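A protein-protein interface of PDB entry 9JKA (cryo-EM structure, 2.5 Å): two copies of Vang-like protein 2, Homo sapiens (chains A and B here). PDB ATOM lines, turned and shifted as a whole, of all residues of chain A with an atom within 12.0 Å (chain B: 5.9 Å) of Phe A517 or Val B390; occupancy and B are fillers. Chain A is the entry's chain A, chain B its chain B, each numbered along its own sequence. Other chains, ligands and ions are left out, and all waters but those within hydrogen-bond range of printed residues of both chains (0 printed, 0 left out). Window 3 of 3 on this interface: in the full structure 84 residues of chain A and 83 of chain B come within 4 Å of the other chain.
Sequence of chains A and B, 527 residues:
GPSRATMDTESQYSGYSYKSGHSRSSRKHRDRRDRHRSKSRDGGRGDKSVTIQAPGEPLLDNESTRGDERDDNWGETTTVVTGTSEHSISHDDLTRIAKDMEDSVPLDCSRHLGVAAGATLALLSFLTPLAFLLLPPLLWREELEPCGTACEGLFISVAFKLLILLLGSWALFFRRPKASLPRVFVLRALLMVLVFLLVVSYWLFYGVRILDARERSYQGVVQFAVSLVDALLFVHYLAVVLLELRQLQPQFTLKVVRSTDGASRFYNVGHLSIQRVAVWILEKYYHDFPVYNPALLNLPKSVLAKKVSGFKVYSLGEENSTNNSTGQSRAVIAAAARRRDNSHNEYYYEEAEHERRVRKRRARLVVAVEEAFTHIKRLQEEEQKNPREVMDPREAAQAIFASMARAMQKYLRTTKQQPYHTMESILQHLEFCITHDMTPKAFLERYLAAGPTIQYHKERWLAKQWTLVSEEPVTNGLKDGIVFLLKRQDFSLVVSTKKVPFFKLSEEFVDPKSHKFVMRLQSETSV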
ATOM      1  N   VAL A 510     -13.969 -10.153   6.141  1.00  0.00           N
ATOM      2  CA  VAL A 510     -14.949 -10.188   7.214  1.00  0.00           C
ATOM      3  C   VAL A 510     -16.288 -10.590   6.618  1.00  0.00           C
ATOM      4  O   VAL A 510     -16.547 -10.405   5.424  1.00  0.00           O
ATOM      5  CB  VAL A 510     -15.062  -8.842   7.963  1.00  0.00           C
ATOM      6  CG1 VAL A 510     -13.746  -8.501   8.638  1.00  0.00           C
ATOM      7  CG2 VAL A 510     -15.490  -7.732   7.019  1.00  0.00           C
ATOM      8  N   ASP A 511     -17.119 -11.159   7.445  1.00  0.00           N
ATOM      9  CA  ASP A 511     -18.460 -11.528   7.018  1.00  0.00           C
ATOM     10  C   ASP A 511     -19.439 -10.450   7.468  1.00  0.00           C
ATOM     11  O   ASP A 511     -19.443 -10.088   8.650  1.00  0.00           O
ATOM     12  CB  ASP A 511     -18.849 -12.877   7.614  1.00  0.00           C
ATOM     13  CG  ASP A 511     -20.067 -13.500   6.947  1.00  0.00           C
ATOM     14  OD1 ASP A 511     -20.612 -12.922   5.986  1.00  0.00           O
ATOM     15  OD2 ASP A 511     -20.488 -14.585   7.396  1.00  0.00           O
ATOM     16  N   PRO A 512     -20.249  -9.891   6.559  1.00  0.00           N
ATOM     17  CA  PRO A 512     -21.313  -8.966   6.992  1.00  0.00           C
ATOM     18  C   PRO A 512     -22.360  -9.606   7.890  1.00  0.00           C
ATOM     19  O   PRO A 512     -23.029  -8.885   8.642  1.00  0.00           O
ATOM     20  CB  PRO A 512     -21.926  -8.495   5.668  1.00  0.00           C
ATOM     21  CG  PRO A 512     -20.822  -8.639   4.683  1.00  0.00           C
ATOM     22  CD  PRO A 512     -20.057  -9.859   5.100  1.00  0.00           C
ATOM     23  N   LYS A 513     -22.525 -10.927   7.835  1.00  0.00           N
ATOM     24  CA  LYS A 513     -23.343 -11.636   8.806  1.00  0.00           C
ATOM     25  C   LYS A 513     -22.699 -11.671  10.187  1.00  0.00           C
ATOM     26  O   LYS A 513     -23.415 -11.689  11.193  1.00  0.00           O
ATOM     27  CB  LYS A 513     -23.606 -13.061   8.302  1.00  0.00           C
ATOM     28  CG  LYS A 513     -24.593 -13.883   9.120  1.00  0.00           C
ATOM     29  CD  LYS A 513     -24.828 -15.245   8.490  1.00  0.00           C
ATOM     30  CE  LYS A 513     -25.797 -16.077   9.313  1.00  0.00           C
ATOM     31  NZ  LYS A 513     -26.027 -17.419   8.709  1.00  0.00           N
ATOM     32  N   SER A 514     -21.368 -11.626  10.263  1.00  0.00           N
ATOM     33  CA  SER A 514     -20.651 -11.803  11.521  1.00  0.00           C
ATOM     34  C   SER A 514     -20.622 -10.557  12.399  1.00  0.00           C
ATOM     35  O   SER A 514     -19.928 -10.563  13.419  1.00  0.00           O
ATOM     36  CB  SER A 514     -19.214 -12.251  11.248  1.00  0.00           C
ATOM     37  OG  SER A 514     -18.483 -11.231  10.590  1.00  0.00           O
ATOM     38  N   HIS A 515     -21.341  -9.495  12.040  1.00  0.00           N
ATOM     39  CA  HIS A 515     -21.413  -8.301  12.877  1.00  0.00           C
ATOM     40  C   HIS A 515     -22.598  -8.471  13.819  1.00  0.00           C
ATOM     41  O   HIS A 515     -23.734  -8.137  13.490  1.00  0.00           O
ATOM     42  CB  HIS A 515     -21.541  -7.045  12.025  1.00  0.00           C
ATOM     43  CG  HIS A 515     -20.383  -6.820  11.104  1.00  0.00           C
ATOM     44  ND1 HIS A 515     -19.141  -6.422  11.550  1.00  0.00           N
ATOM     45  CD2 HIS A 515     -20.280  -6.929   9.759  1.00  0.00           C
ATOM     46  CE1 HIS A 515     -18.322  -6.304  10.521  1.00  0.00           C
ATOM     47  NE2 HIS A 515     -18.989  -6.603   9.422  1.00  0.00           N
ATOM     48  N   LYS A 516     -22.327  -9.002  15.008  1.00  0.00           N
ATOM     49  CA  LYS A 516     -23.352  -9.263  16.007  1.00  0.00           C
ATOM     50  C   LYS A 516     -23.053  -8.467  17.267  1.00  0.00           C
ATOM     51  O   LYS A 516     -21.889  -8.219  17.593  1.00  0.00           O
ATOM     52  CB  LYS A 516     -23.445 -10.754  16.329  1.00  0.00           C
ATOM     53  CG  LYS A 516     -23.847 -11.605  15.139  1.00  0.00           C
ATOM     54  CD  LYS A 516     -25.248 -11.243  14.677  1.00  0.00           C
ATOM     55  CE  LYS A 516     -25.709 -12.130  13.538  1.00  0.00           C
ATOM     56  NZ  LYS A 516     -27.059 -11.733  13.049  1.00  0.00           N
ATOM     57  N   PHE A 517     -24.111  -8.094  17.983  1.00  0.00           N
ATOM     58  CA  PHE A 517     -24.055  -7.078  19.021  1.00  0.00           C
ATOM     59  C   PHE A 517     -24.848  -7.503  20.249  1.00  0.00           C
ATOM     60  O   PHE A 517     -25.778  -8.309  20.171  1.00  0.00           O
ATOM     61  CB  PHE A 517     -24.587  -5.748  18.475  1.00  0.00           C
ATOM     62  CG  PHE A 517     -23.636  -5.061  17.552  1.00  0.00           C
ATOM     63  CD1 PHE A 517     -22.280  -5.091  17.799  1.00  0.00           C
ATOM     64  CD2 PHE A 517     -24.081  -4.493  16.377  1.00  0.00           C
ATOM     65  CE1 PHE A 517     -21.403  -4.491  16.944  1.00  0.00           C
ATOM     66  CE2 PHE A 517     -23.199  -3.902  15.514  1.00  0.00           C
ATOM     67  CZ  PHE A 517     -21.861  -3.905  15.798  1.00  0.00           C
ATOM     68  N   VAL A 518     -24.448  -6.961  21.398  1.00  0.00           N
ATOM     69  CA  VAL A 518     -25.137  -7.165  22.665  1.00  0.00           C
ATOM     70  C   VAL A 518     -25.483  -5.802  23.240  1.00  0.00           C
ATOM     71  O   VAL A 518     -25.105  -4.764  22.690  1.00  0.00           O
ATOM     72  CB  VAL A 518     -24.291  -7.979  23.668  1.00  0.00           C
ATOM     73  CG1 VAL A 518     -24.032  -9.378  23.140  1.00  0.00           C
ATOM     74  CG2 VAL A 518     -22.986  -7.263  23.958  1.00  0.00           C
ATOM     75  N   MET A 519     -26.217  -5.805  24.352  1.00  0.00           N
ATOM     76  CA  MET A 519     -26.673  -4.574  24.987  1.00  0.00           C
ATOM     77  C   MET A 519     -25.811  -4.189  26.195  1.00  0.00           C
ATOM     78  O   MET A 519     -25.979  -3.109  26.775  1.00  0.00           O
ATOM     79  CB  MET A 519     -28.150  -4.730  25.370  1.00  0.00           C
ATOM     80  CG  MET A 519     -28.927  -3.451  25.702  1.00  0.00           C
ATOM     81  SD  MET A 519     -29.064  -2.313  24.313  1.00  0.00           S
ATOM     82  CE  MET A 519     -30.288  -3.158  23.320  1.00  0.00           C
ATOM     83  N   ARG A 520     -24.841  -5.016  26.560  1.00  0.00           N
ATOM     84  CA  ARG A 520     -24.057  -4.793  27.765  1.00  0.00           C
ATOM     85  C   ARG A 520     -22.729  -4.143  27.410  1.00  0.00           C
ATOM     86  O   ARG A 520     -21.944  -4.718  26.648  1.00  0.00           O
ATOM     87  CB  ARG A 520     -23.816  -6.103  28.517  1.00  0.00           C
ATOM     88  CG  ARG A 520     -22.996  -5.930  29.776  1.00  0.00           C
ATOM     89  CD  ARG A 520     -23.739  -5.066  30.775  1.00  0.00           C
ATOM     90  NE  ARG A 520     -24.962  -5.711  31.237  1.00  0.00           N
ATOM     91  CZ  ARG A 520     -25.927  -5.086  31.902  1.00  0.00           C
ATOM     92  NH1 ARG A 520     -25.813  -3.794  32.181  1.00  0.00           N
ATOM     93  NH2 ARG A 520     -27.006  -5.752  32.287  1.00  0.00           N
ATOM     94  N   LEU A 521     -22.495  -2.951  27.966  1.00  0.00           N
ATOM     95  CA  LEU A 521     -21.231  -2.203  27.889  1.00  0.00           C
ATOM     96  C   LEU A 521     -20.818  -1.903  26.449  1.00  0.00           C
ATOM     97  O   LEU A 521     -20.143  -0.909  26.182  1.00  0.00           O
ATOM     98  CB  LEU A 521     -20.120  -2.967  28.640  1.00  0.00           C
ATOM     99  CG  LEU A 521     -18.759  -2.354  29.016  1.00  0.00           C
ATOM    100  CD1 LEU A 521     -17.711  -2.398  27.899  1.00  0.00           C
ATOM    101  CD2 LEU A 521     -18.948  -0.927  29.516  1.00  0.00           C
ATOM    102  N   ILE B 376     -23.602  -0.624  23.404  1.00  0.00           N
ATOM    103  CA  ILE B 376     -23.438  -1.853  22.638  1.00  0.00           C
ATOM    104  C   ILE B 376     -21.980  -2.289  22.669  1.00  0.00           C
ATOM    105  O   ILE B 376     -21.084  -1.539  23.054  1.00  0.00           O
ATOM    106  CB  ILE B 376     -23.922  -1.720  21.178  1.00  0.00           C
ATOM    107  CG1 ILE B 376     -23.272  -0.513  20.502  1.00  0.00           C
ATOM    108  CG2 ILE B 376     -25.442  -1.711  21.091  1.00  0.00           C
ATOM    109  CD1 ILE B 376     -23.513  -0.455  19.027  1.00  0.00           C
ATOM    110  N   LYS B 377     -21.759  -3.529  22.239  1.00  0.00           N
ATOM    111  CA  LYS B 377     -20.449  -4.157  22.227  1.00  0.00           C
ATOM    112  C   LYS B 377     -20.472  -5.260  21.179  1.00  0.00           C
ATOM    113  O   LYS B 377     -21.535  -5.798  20.864  1.00  0.00           O
ATOM    114  CB  LYS B 377     -20.099  -4.714  23.621  1.00  0.00           C
ATOM    115  CG  LYS B 377     -18.667  -5.193  23.819  1.00  0.00           C
ATOM    116  CD  LYS B 377     -18.437  -5.708  25.228  1.00  0.00           C
ATOM    117  CE  LYS B 377     -17.011  -6.213  25.391  1.00  0.00           C
ATOM    118  NZ  LYS B 377     -16.751  -6.740  26.757  1.00  0.00           N
ATOM    119  N   ARG B 378     -19.298  -5.579  20.629  1.00  0.00           N
ATOM    120  CA  ARG B 378     -19.167  -6.658  19.655  1.00  0.00           C
ATOM    121  C   ARG B 378     -19.526  -8.008  20.271  1.00  0.00           C
ATOM    122  O   ARG B 378     -19.523  -8.178  21.492  1.00  0.00           O
ATOM    123  CB  ARG B 378     -17.732  -6.721  19.128  1.00  0.00           C
ATOM    124  CG  ARG B 378     -17.208  -5.471  18.444  1.00  0.00           C
ATOM    125  CD  ARG B 378     -17.802  -5.256  17.070  1.00  0.00           C
ATOM    126  NE  ARG B 378     -17.453  -6.324  16.141  1.00  0.00           N
ATOM    127  CZ  ARG B 378     -18.021  -6.489  14.950  1.00  0.00           C
ATOM    128  NH1 ARG B 378     -18.949  -5.641  14.535  1.00  0.00           N
ATOM    129  NH2 ARG B 378     -17.650  -7.491  14.165  1.00  0.00           N
ATOM    130  N   LEU B 379     -19.818  -8.978  19.412  1.00  0.00           N
ATOM    131  CA  LEU B 379     -20.074 -10.339  19.862  1.00  0.00           C
ATOM    132  C   LEU B 379     -19.313 -11.345  19.009  1.00  0.00           C
ATOM    133  O   LEU B 379     -18.422 -10.974  18.244  1.00  0.00           O
ATOM    134  CB  LEU B 379     -21.569 -10.646  19.830  1.00  0.00           C
ATOM    135  CG  LEU B 379     -21.971 -12.048  20.285  1.00  0.00           C
ATOM    136  CD1 LEU B 379     -21.575 -12.272  21.734  1.00  0.00           C
ATOM    137  CD2 LEU B 379     -23.464 -12.267  20.087  1.00  0.00           C
ATOM    138  N   VAL B 390     -27.434 -11.823  20.605  1.00  0.00           N
ATOM    139  CA  VAL B 390     -27.432 -11.624  19.163  1.00  0.00           C
ATOM    140  C   VAL B 390     -28.364 -10.467  18.783  1.00  0.00           C
ATOM    141  O   VAL B 390     -29.500 -10.376  19.257  1.00  0.00           O
ATOM    142  CB  VAL B 390     -27.779 -12.956  18.423  1.00  0.00           C
ATOM    143  CG1 VAL B 390     -29.107 -13.551  18.896  1.00  0.00           C
ATOM    144  CG2 VAL B 390     -27.787 -12.757  16.914  1.00  0.00           C
ATOM    145  N   MET B 391     -27.848  -9.560  17.955  1.00  0.00           N
ATOM    146  CA  MET B 391     -28.550  -8.352  17.546  1.00  0.00           C
ATOM    147  C   MET B 391     -27.880  -7.778  16.303  1.00  0.00           C
ATOM    148  O   MET B 391     -26.657  -7.610  16.275  1.00  0.00           O
ATOM    149  CB  MET B 391     -28.573  -7.329  18.689  1.00  0.00           C
ATOM    150  CG  MET B 391     -29.272  -6.029  18.386  1.00  0.00           C
ATOM    151  SD  MET B 391     -29.522  -5.063  19.882  1.00  0.00           S
ATOM    152  CE  MET B 391     -27.841  -4.687  20.354  1.00  0.00           C
ATOM    153  N   ASP B 392     -28.687  -7.503  15.279  1.00  0.00           N
ATOM    154  CA  ASP B 392     -28.196  -6.969  14.016  1.00  0.00           C
ATOM    155  C   ASP B 392     -27.641  -5.555  14.201  1.00  0.00           C
ATOM    156  O   ASP B 392     -28.024  -4.855  15.142  1.00  0.00           O
ATOM    157  CB  ASP B 392     -29.326  -6.951  12.986  1.00  0.00           C
ATOM    158  CG  ASP B 392     -29.684  -8.333  12.488  1.00  0.00           C
ATOM    159  OD1 ASP B 392     -28.786  -9.199  12.444  1.00  0.00           O
ATOM    160  OD2 ASP B 392     -30.863  -8.555  12.141  1.00  0.00           O
ATOM    161  N   PRO B 393     -26.724  -5.118  13.329  1.00  0.00           N
ATOM    162  CA  PRO B 393     -26.280  -3.714  13.386  1.00  0.00           C
ATOM    163  C   PRO B 393     -27.376  -2.715  13.068  1.00  0.00           C
ATOM    164  O   PRO B 393     -27.326  -1.591  13.577  1.00  0.00           O
ATOM    165  CB  PRO B 393     -25.147  -3.659  12.352  1.00  0.00           C
ATOM    166  CG  PRO B 393     -25.388  -4.807  11.455  1.00  0.00           C
ATOM    167  CD  PRO B 393     -25.965  -5.879  12.321  1.00  0.00           C
ATOM    168  N   GLU B 395     -30.525  -3.313  14.076  1.00  0.00           N
ATOM    169  CA  GLU B 395     -31.232  -3.331  15.350  1.00  0.00           C
ATOM    170  C   GLU B 395     -30.438  -2.638  16.446  1.00  0.00           C
ATOM    171  O   GLU B 395     -31.023  -1.953  17.292  1.00  0.00           O
ATOM    172  CB  GLU B 395     -31.540  -4.769  15.753  1.00  0.00           C
ATOM    173  CG  GLU B 395     -32.507  -5.472  14.831  1.00  0.00           C
ATOM    174  CD  GLU B 395     -32.761  -6.904  15.245  1.00  0.00           C
ATOM    175  OE1 GLU B 395     -32.087  -7.381  16.181  1.00  0.00           O
ATOM    176  OE2 GLU B 395     -33.634  -7.554  14.632  1.00  0.00           O
ATOM    177  N   ALA B 396     -29.112  -2.773  16.430  1.00  0.00           N
ATOM    178  CA  ALA B 396     -28.292  -2.099  17.431  1.00  0.00           C
ATOM    179  C   ALA B 396     -28.268  -0.596  17.207  1.00  0.00           C
ATOM    180  O   ALA B 396     -28.281   0.178  18.170  1.00  0.00           O
ATOM    181  CB  ALA B 396     -26.874  -2.656  17.409  1.00  0.00           C
ATOM    182  N   ILE B 434     -21.181   1.490  13.387  1.00  0.00           N
ATOM    183  CA  ILE B 434     -20.972   0.388  14.318  1.00  0.00           C
ATOM    184  C   ILE B 434     -20.600  -0.893  13.587  1.00  0.00           C
ATOM    185  O   ILE B 434     -19.994  -1.782  14.195  1.00  0.00           O
ATOM    186  CB  ILE B 434     -22.199   0.171  15.222  1.00  0.00           C
ATOM    187  CG1 ILE B 434     -23.400  -0.320  14.423  1.00  0.00           C
ATOM    188  CG2 ILE B 434     -22.544   1.455  15.952  1.00  0.00           C
ATOM    189  CD1 ILE B 434     -24.597  -0.610  15.268  1.00  0.00           C
ATOM    190  N   THR B 435     -20.912  -1.002  12.292  1.00  0.00           N
ATOM    191  CA  THR B 435     -20.449  -2.146  11.515  1.00  0.00           C
ATOM    192  C   THR B 435     -18.939  -2.102  11.318  1.00  0.00           C
ATOM    193  O   THR B 435     -18.252  -3.115  11.488  1.00  0.00           O
ATOM    194  CB  THR B 435     -21.171  -2.181  10.169  1.00  0.00           C
ATOM    195  OG1 THR B 435     -22.580  -2.288  10.387  1.00  0.00           O
ATOM    196  CG2 THR B 435     -20.713  -3.357   9.336  1.00  0.00           C
ATOM    197  N   ASP B 437     -16.724  -0.455  13.097  1.00  0.00           N
ATOM    198  CA  ASP B 437     -16.044  -0.189  14.373  1.00  0.00           C
ATOM    199  C   ASP B 437     -15.575   1.260  14.485  1.00  0.00           C
ATOM    200  O   ASP B 437     -14.466   1.539  14.945  1.00  0.00           O
ATOM    201  CB  ASP B 437     -14.883  -1.158  14.605  1.00  0.00           C
ATOM    202  CG  ASP B 437     -15.353  -2.572  14.850  1.00  0.00           C
ATOM    203  OD1 ASP B 437     -16.471  -2.738  15.377  1.00  0.00           O
ATOM    204  OD2 ASP B 437     -14.609  -3.516  14.515  1.00  0.00           O
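Ser A514 touches Arg B378 (O to NH2, 3.9 Å).
Pro B393 touches His A515.
O of Lys A516 touches C of Arg B378 (3.6 Å).
CG2 of Val B390 touches CD of Lys A516 (3.7 Å).
NH1 of Arg B378 touches CZ of Phe A517, at 3.6 Å.
Phe A517 touches Val B390 (O to C, 3.6 Å).
Ala B396 touches Phe A517.
CZ of Phe A517 touches O of Ile B434 (3.2 Å).
Ile B376 touches Val A518 (CA to O, 3.4 Å).
CB of Lys B377 touches O of Arg A520, 3.5 Å away.
No position is printed for both chains.
Of the 21 pairs that touch across the chains among the printed residues, none has its exchanged pair printed and touching as well.
Of the 12 printed residues of chain A, 7 touch a printed residue of chain B.
Printed residues of chain A that touch a printed residue of chain B: Ser A514, His A515, Lys A516, Phe A517, Val A518, Arg A520 and Leu A521.
Printed residues of chain B that touch a printed residue of chain A: Ile B376, Lys B377, Arg B378, Leu B379, Val B390, Met B391, Asp B392, Pro B393, Ala B396, Ile B434 and Thr B435.
Among the printed residues, Asp or Glu carboxylates within 4 Å of a Lys or Arg side-chain nitrogen of the other chain: Lys A516 with Asp B392 (3.1 Å).
O of Asp A511 sits at hydrogen-bond distance from OG of Ser A514 (2.4 Å).
OD1 of Asp B437 is in salt-bridge range of NE of Arg B378 (3.8 Å).
N of Leu B379 lies within hydrogen-bond range of O of Lys A516, 2.9 Å away.
The guanidinium group (NH1) of Arg B378 is in hydrogen-bond range of a ring nitrogen (ND1) of His A515, 3.1 Å away.
The backbone carbonyl oxygen of Thr B435 sits close to a ring nitrogen (ND1) of His A515.
O of Lys B377 sits at hydrogen-bond distance from N of Val A518, at 3.2 Å.
The side-chain amino group (NZ) of Lys A516 lies within salt-bridge range of the side-chain carboxylate (OD1) of Asp B392 (3.1 Å).
The backbone carbonyl oxygen (O) of Ile B376 lies close to the backbone carbonyl oxygen (O) of Leu A521 (3.3 Å).
The backbone carbonyl oxygen of Met B391 lies within hydrogen-bond range of the backbone NH of Phe A517 (3.1 Å).
Asp A511 touches none of the printed residues of chain B.
Of the printed residues of chain B, Ser A514 touches Arg B378.
Of chain B, only Lys B377 (3.2 Å), Arg B378 (3.6 Å), Val B390 (3.6 Å), Met B391 (3.1 Å), Pro B393 (3.7 Å), Ala B396 (3.5 Å) and Ile B434 (3.2 Å) come within 4 Å of Phe A517.
Of the printed residues of chain B, Val A518 touches Ile B376, Lys B377 and Met B391.
Printed residues of chain B within 4 Å of Arg A520: Lys B377.
Of chain A, only Val A518 and Leu A521 come within 4 Å of Ile B376.
Of the printed residues of chain A, Lys B377 touches Phe A517 (3.2 Å), Val A518 (3.2 Å) and Arg A520 (3.5 Å).
Of chain A, only Ser A514 (3.9 Å), His A515 (3.1 Å), Lys A516 (3.6 Å) and Phe A517 (3.6 Å) come within 4 Å of Arg B378.
Of chain A, only Lys A516 comes within 4 Å of Leu B379.
Val B390 touches just these residues of chain A: Lys A516 and Phe A517.
Of chain A, only Lys A516 (3.1 Å) comes within 4 Å of Asp B392.
No residue of chain A comes within 4 Å of Glu B395.
Of chain A, only Phe A517 comes within 4 Å of Ala B396.
Ile B434 touches just one residue of chain A: Phe A517 (3.2 Å).
Of chain A, only His A515 (3.3 Å) comes within 4 Å of Thr B435.
The nearest residue of chain A that does not touch Val B390 is Val A518 (4.9 Å).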
